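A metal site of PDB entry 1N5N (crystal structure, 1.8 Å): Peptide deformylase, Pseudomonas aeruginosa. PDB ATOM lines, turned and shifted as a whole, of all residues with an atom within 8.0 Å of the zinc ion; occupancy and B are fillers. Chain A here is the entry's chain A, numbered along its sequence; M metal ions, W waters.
ND1 of His 146 is in hydrogen-bond range of OE1 of Glu 102 (2.8 Å). The backbone NH (N) of Ser 106 lies close to the side-chain sulfur (SG) of Cys 104 (3.3 Å). OE1 of Glu 147 sits close to OE1 of Gln 63 (3.3 Å). NE2 of Gln 63 lies within hydrogen-bond range of OG of Ser 106. The side-chain amide oxygen (OE1) of Gln 63 is in hydrogen-bond range of the backbone NH (N) of Ala 60, 2.8 Å away.
Residues that only touch the zinc ion: Gln 63 (3.6 Å).
NE2 of His 146 binds the zinc ion (2.0 Å). NE2 of His 150 is bound to the zinc ion (2.0 Å). Water W1 binds the zinc ion, 2.2 Å away. The zinc ion is bound by the side-chain sulfur (SG) of Cys 104 (2.3 Å).
Water W1 lies within hydrogen-bond range of the side-chain carboxylate of Glu 147 (3.2 Å), the side-chain amide nitrogen of Gln 63 (3.3 Å) and the backbone NH of Leu 105 (3.4 Å).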
ATOM      1  N   ILE A  18     -11.842  14.679  -5.919  1.00  0.00           N
ATOM      2  CA  ILE A  18     -11.219  14.505  -7.244  1.00  0.00           C
ATOM      3  C   ILE A  18     -11.420  15.823  -7.980  1.00  0.00           C
ATOM      4  O   ILE A  18     -12.604  16.302  -8.057  1.00  0.00           O
ATOM      5  CB  ILE A  18     -11.992  13.456  -7.980  1.00  0.00           C
ATOM      6  CG1 ILE A  18     -11.805  12.146  -7.195  1.00  0.00           C
ATOM      7  CG2 ILE A  18     -11.557  13.277  -9.409  1.00  0.00           C
ATOM      8  CD1 ILE A  18     -12.782  10.961  -7.856  1.00  0.00           C
ATOM      9  N   LEU A  26      -5.219  20.225 -12.833  1.00  0.00           N
ATOM     10  CA  LEU A  26      -5.160  18.955 -13.530  1.00  0.00           C
ATOM     11  C   LEU A  26      -4.107  19.081 -14.605  1.00  0.00           C
ATOM     12  O   LEU A  26      -3.821  18.124 -15.327  1.00  0.00           O
ATOM     13  CB  LEU A  26      -6.516  18.675 -14.208  1.00  0.00           C
ATOM     14  CG  LEU A  26      -7.570  18.163 -13.214  1.00  0.00           C
ATOM     15  CD1 LEU A  26      -9.043  18.138 -13.852  1.00  0.00           C
ATOM     16  CD2 LEU A  26      -6.982  16.637 -12.852  1.00  0.00           C
ATOM     17  N   GLY A  58      -9.640   3.704 -12.691  1.00  0.00           N
ATOM     18  CA  GLY A  58      -8.239   4.133 -12.694  1.00  0.00           C
ATOM     19  C   GLY A  58      -8.231   5.507 -12.050  1.00  0.00           C
ATOM     20  O   GLY A  58      -9.228   6.219 -12.070  1.00  0.00           O
ATOM     21  N   LEU A  59      -7.125   5.834 -11.396  1.00  0.00           N
ATOM     22  CA  LEU A  59      -7.129   7.165 -10.798  1.00  0.00           C
ATOM     23  C   LEU A  59      -5.573   7.577 -10.712  1.00  0.00           C
ATOM     24  O   LEU A  59      -4.775   6.761 -10.357  1.00  0.00           O
ATOM     25  CB  LEU A  59      -7.699   7.114  -9.370  1.00  0.00           C
ATOM     26  CG  LEU A  59      -7.644   8.521  -8.626  1.00  0.00           C
ATOM     27  CD1 LEU A  59      -8.588   9.564  -9.345  1.00  0.00           C
ATOM     28  CD2 LEU A  59      -8.053   8.311  -7.163  1.00  0.00           C
ATOM     29  N   ALA A  60      -5.251   8.767 -11.188  1.00  0.00           N
ATOM     30  CA  ALA A  60      -3.815   9.258 -11.081  1.00  0.00           C
ATOM     31  C   ALA A  60      -3.758  10.270  -9.916  1.00  0.00           C
ATOM     32  O   ALA A  60      -4.717  10.960  -9.621  1.00  0.00           O
ATOM     33  CB  ALA A  60      -3.387  10.037 -12.478  1.00  0.00           C
ATOM     34  N   GLN A  63      -5.108  13.790 -10.134  1.00  0.00           N
ATOM     35  CA  GLN A  63      -6.502  14.075  -9.952  1.00  0.00           C
ATOM     36  C   GLN A  63      -6.960  14.318  -8.580  1.00  0.00           C
ATOM     37  O   GLN A  63      -8.069  14.728  -8.466  1.00  0.00           O
ATOM     38  CB  GLN A  63      -7.338  12.853 -10.460  1.00  0.00           C
ATOM     39  CG  GLN A  63      -7.070  12.611 -12.031  1.00  0.00           C
ATOM     40  CD  GLN A  63      -7.793  11.336 -12.510  1.00  0.00           C
ATOM     41  OE1 GLN A  63      -7.223  10.250 -12.513  1.00  0.00           O
ATOM     42  NE2 GLN A  63      -9.106  11.477 -12.806  1.00  0.00           N
ATOM     43  N   GLU A 102     -13.763   6.654 -23.949  1.00  0.00           N
ATOM     44  CA  GLU A 102     -13.294   6.819 -22.603  1.00  0.00           C
ATOM     45  C   GLU A 102     -14.073   7.755 -21.785  1.00  0.00           C
ATOM     46  O   GLU A 102     -14.667   8.764 -22.316  1.00  0.00           O
ATOM     47  CB  GLU A 102     -11.830   7.379 -22.662  1.00  0.00           C
ATOM     48  CG  GLU A 102     -10.970   6.478 -23.286  1.00  0.00           C
ATOM     49  CD  GLU A 102      -9.358   6.933 -23.316  1.00  0.00           C
ATOM     50  OE1 GLU A 102      -9.062   7.842 -22.554  1.00  0.00           O
ATOM     51  OE2 GLU A 102      -8.675   6.390 -24.138  1.00  0.00           O
ATOM     52  N   GLY A 103     -14.038   7.497 -20.496  1.00  0.00           N
ATOM     53  CA  GLY A 103     -14.523   8.516 -19.601  1.00  0.00           C
ATOM     54  C   GLY A 103     -13.373   8.838 -18.629  1.00  0.00           C
ATOM     55  O   GLY A 103     -12.218   8.370 -18.761  1.00  0.00           O
ATOM     56  N   CYS A 104     -13.661   9.642 -17.605  1.00  0.00           N
ATOM     57  CA  CYS A 104     -12.644  10.094 -16.733  1.00  0.00           C
ATOM     58  C   CYS A 104     -13.316  10.579 -15.469  1.00  0.00           C
ATOM     59  O   CYS A 104     -14.315  11.367 -15.528  1.00  0.00           O
ATOM     60  CB  CYS A 104     -11.929  11.307 -17.383  1.00  0.00           C
ATOM     61  SG  CYS A 104     -10.571  11.956 -16.328  1.00  0.00           S
ATOM     62  N   LEU A 105     -12.758  10.244 -14.310  1.00  0.00           N
ATOM     63  CA  LEU A 105     -13.365  10.738 -13.092  1.00  0.00           C
ATOM     64  C   LEU A 105     -13.252  12.279 -13.000  1.00  0.00           C
ATOM     65  O   LEU A 105     -14.027  12.890 -12.260  1.00  0.00           O
ATOM     66  CB  LEU A 105     -12.689  10.184 -11.824  1.00  0.00           C
ATOM     67  CG  LEU A 105     -12.812   8.602 -11.874  1.00  0.00           C
ATOM     68  CD1 LEU A 105     -12.096   7.943 -10.659  1.00  0.00           C
ATOM     69  CD2 LEU A 105     -14.321   8.358 -11.741  1.00  0.00           C
ATOM     70  N   SER A 106     -12.283  12.873 -13.690  1.00  0.00           N
ATOM     71  CA  SER A 106     -12.231  14.362 -13.634  1.00  0.00           C
ATOM     72  C   SER A 106     -13.008  15.005 -14.809  1.00  0.00           C
ATOM     73  O   SER A 106     -12.941  16.258 -14.826  1.00  0.00           O
ATOM     74  CB  SER A 106     -10.716  14.773 -13.772  1.00  0.00           C
ATOM     75  OG  SER A 106      -9.964  14.332 -12.632  1.00  0.00           O
ATOM     76  N   VAL A 107     -13.865  14.274 -15.606  1.00  0.00           N
ATOM     77  CA  VAL A 107     -14.653  14.830 -16.684  1.00  0.00           C
ATOM     78  C   VAL A 107     -15.909  13.988 -16.529  1.00  0.00           C
ATOM     79  O   VAL A 107     -16.354  13.267 -17.437  1.00  0.00           O
ATOM     80  CB  VAL A 107     -14.018  14.667 -18.066  1.00  0.00           C
ATOM     81  CG1 VAL A 107     -14.793  15.623 -19.074  1.00  0.00           C
ATOM     82  CG2 VAL A 107     -12.442  15.114 -18.113  1.00  0.00           C
ATOM     83  N   ARG A 116      -5.963   5.196 -29.425  1.00  0.00           N
ATOM     84  CA  ARG A 116      -4.670   5.080 -28.810  1.00  0.00           C
ATOM     85  C   ARG A 116      -4.067   3.766 -29.315  1.00  0.00           C
ATOM     86  O   ARG A 116      -4.790   2.852 -29.722  1.00  0.00           O
ATOM     87  CB  ARG A 116      -4.764   4.899 -27.261  1.00  0.00           C
ATOM     88  CG  ARG A 116      -5.385   6.097 -26.633  1.00  0.00           C
ATOM     89  CD  ARG A 116      -5.316   5.902 -25.062  1.00  0.00           C
ATOM     90  NE  ARG A 116      -6.063   6.983 -24.392  1.00  0.00           N
ATOM     91  CZ  ARG A 116      -5.623   8.097 -23.851  1.00  0.00           C
ATOM     92  NH1 ARG A 116      -4.328   8.428 -23.890  1.00  0.00           N
ATOM     93  NH2 ARG A 116      -6.477   8.746 -23.062  1.00  0.00           N
ATOM     94  N   CYS A 143      -6.215   2.142 -20.183  1.00  0.00           N
ATOM     95  CA  CYS A 143      -6.202   2.797 -18.853  1.00  0.00           C
ATOM     96  C   CYS A 143      -4.835   3.320 -18.544  1.00  0.00           C
ATOM     97  O   CYS A 143      -4.677   4.454 -18.019  1.00  0.00           O
ATOM     98  CB  CYS A 143      -6.728   1.776 -17.817  1.00  0.00           C
ATOM     99  SG  CYS A 143      -7.124   2.598 -16.116  1.00  0.00           S
ATOM    100  N   HIS A 146      -4.296   6.476 -20.533  1.00  0.00           N
ATOM    101  CA  HIS A 146      -5.094   7.559 -20.043  1.00  0.00           C
ATOM    102  C   HIS A 146      -4.471   8.080 -18.708  1.00  0.00           C
ATOM    103  O   HIS A 146      -4.509   9.286 -18.454  1.00  0.00           O
ATOM    104  CB  HIS A 146      -6.478   7.011 -19.797  1.00  0.00           C
ATOM    105  CG  HIS A 146      -7.480   7.972 -19.146  1.00  0.00           C
ATOM    106  ND1 HIS A 146      -8.560   8.466 -19.839  1.00  0.00           N
ATOM    107  CD2 HIS A 146      -7.603   8.465 -17.850  1.00  0.00           C
ATOM    108  CE1 HIS A 146      -9.302   9.251 -19.019  1.00  0.00           C
ATOM    109  NE2 HIS A 146      -8.748   9.253 -17.814  1.00  0.00           N
ATOM    110  N   GLU A 147      -4.169   7.173 -17.758  1.00  0.00           N
ATOM    111  CA  GLU A 147      -3.667   7.638 -16.450  1.00  0.00           C
ATOM    112  C   GLU A 147      -2.276   8.233 -16.520  1.00  0.00           C
ATOM    113  O   GLU A 147      -2.019   9.243 -15.823  1.00  0.00           O
ATOM    114  CB  GLU A 147      -3.647   6.504 -15.501  1.00  0.00           C
ATOM    115  CG  GLU A 147      -5.000   5.857 -15.218  1.00  0.00           C
ATOM    116  CD  GLU A 147      -6.126   6.839 -14.773  1.00  0.00           C
ATOM    117  OE1 GLU A 147      -5.776   7.835 -14.197  1.00  0.00           O
ATOM    118  OE2 GLU A 147      -7.363   6.632 -14.926  1.00  0.00           O
ATOM    119  N   ASP A 149      -1.287   9.859 -19.031  1.00  0.00           N
ATOM    120  CA  ASP A 149      -1.545  11.259 -19.544  1.00  0.00           C
ATOM    121  C   ASP A 149      -1.869  12.209 -18.425  1.00  0.00           C
ATOM    122  O   ASP A 149      -1.305  13.326 -18.366  1.00  0.00           O
ATOM    123  CB  ASP A 149      -2.757  11.252 -20.504  1.00  0.00           C
ATOM    124  CG  ASP A 149      -2.412  10.912 -21.898  1.00  0.00           C
ATOM    125  OD1 ASP A 149      -1.208  10.734 -22.216  1.00  0.00           O
ATOM    126  OD2 ASP A 149      -3.360  10.753 -22.735  1.00  0.00           O
ATOM    127  N   HIS A 150      -2.644  11.735 -17.417  1.00  0.00           N
ATOM    128  CA  HIS A 150      -2.919  12.609 -16.291  1.00  0.00           C
ATOM    129  C   HIS A 150      -1.688  13.138 -15.624  1.00  0.00           C
ATOM    130  O   HIS A 150      -1.603  14.307 -15.250  1.00  0.00           O
ATOM    131  CB  HIS A 150      -3.763  11.986 -15.176  1.00  0.00           C
ATOM    132  CG  HIS A 150      -5.192  11.924 -15.527  1.00  0.00           C
ATOM    133  ND1 HIS A 150      -5.976  13.101 -15.624  1.00  0.00           N
ATOM    134  CD2 HIS A 150      -6.073  10.878 -15.673  1.00  0.00           C
ATOM    135  CE1 HIS A 150      -7.262  12.759 -15.792  1.00  0.00           C
ATOM    136  NE2 HIS A 150      -7.350  11.446 -15.841  1.00  0.00           N
ATOM    137  N   LYS A 154      -2.236  15.926 -19.055  1.00  0.00           N
ATOM    138  CA  LYS A 154      -3.148  15.870 -20.195  1.00  0.00           C
ATOM    139  C   LYS A 154      -4.469  15.103 -19.867  1.00  0.00           C
ATOM    140  O   LYS A 154      -4.525  14.161 -19.101  1.00  0.00           O
ATOM    141  CB  LYS A 154      -2.639  15.078 -21.429  1.00  0.00           C
ATOM    142  CG  LYS A 154      -1.324  15.575 -21.910  1.00  0.00           C
ATOM    143  CD  LYS A 154      -0.999  14.605 -23.020  1.00  0.00           C
ATOM    144  CE  LYS A 154       0.349  14.949 -23.658  1.00  0.00           C
ATOM    145  NZ  LYS A 154       0.229  16.040 -24.686  1.00  0.00           N
ATOM    146  N   LEU A 155      -5.496  15.491 -20.566  1.00  0.00           N
ATOM    147  CA  LEU A 155      -6.862  14.888 -20.328  1.00  0.00           C
ATOM    148  C   LEU A 155      -7.389  14.367 -21.555  1.00  0.00           C
ATOM    149  O   LEU A 155      -7.014  14.819 -22.689  1.00  0.00           O
ATOM    150  CB  LEU A 155      -7.859  16.005 -19.892  1.00  0.00           C
ATOM    151  CG  LEU A 155      -7.326  16.732 -18.646  1.00  0.00           C
ATOM    152  CD1 LEU A 155      -8.388  18.006 -18.396  1.00  0.00           C
ATOM    153  CD2 LEU A 155      -7.517  15.815 -17.389  1.00  0.00           C
ATOM    154  N   PHE A 156      -8.316  13.407 -21.457  1.00  0.00           N
ATOM    155  CA  PHE A 156      -8.692  12.884 -22.737  1.00  0.00           C
ATOM    156  C   PHE A 156      -9.490  13.820 -23.686  1.00  0.00           C
ATOM    157  O   PHE A 156      -9.526  13.592 -24.884  1.00  0.00           O
ATOM    158  CB  PHE A 156      -9.461  11.595 -22.558  1.00  0.00           C
ATOM    159  CG  PHE A 156     -10.942  11.762 -22.199  1.00  0.00           C
ATOM    160  CD1 PHE A 156     -11.891  11.742 -23.254  1.00  0.00           C
ATOM    161  CD2 PHE A 156     -11.393  11.996 -20.933  1.00  0.00           C
ATOM    162  CE1 PHE A 156     -13.346  12.000 -22.999  1.00  0.00           C
ATOM    163  CE2 PHE A 156     -12.862  12.223 -20.583  1.00  0.00           C
ATOM    164  CZ  PHE A 156     -13.802  12.233 -21.650  1.00  0.00           C
HETATM  165 ZN    ZN M   1      -9.009  10.321 -16.196  1.00  0.00          ZN
HETATM  166  O   HOH W   1      -9.641   8.828 -14.681  1.00  0.00           O
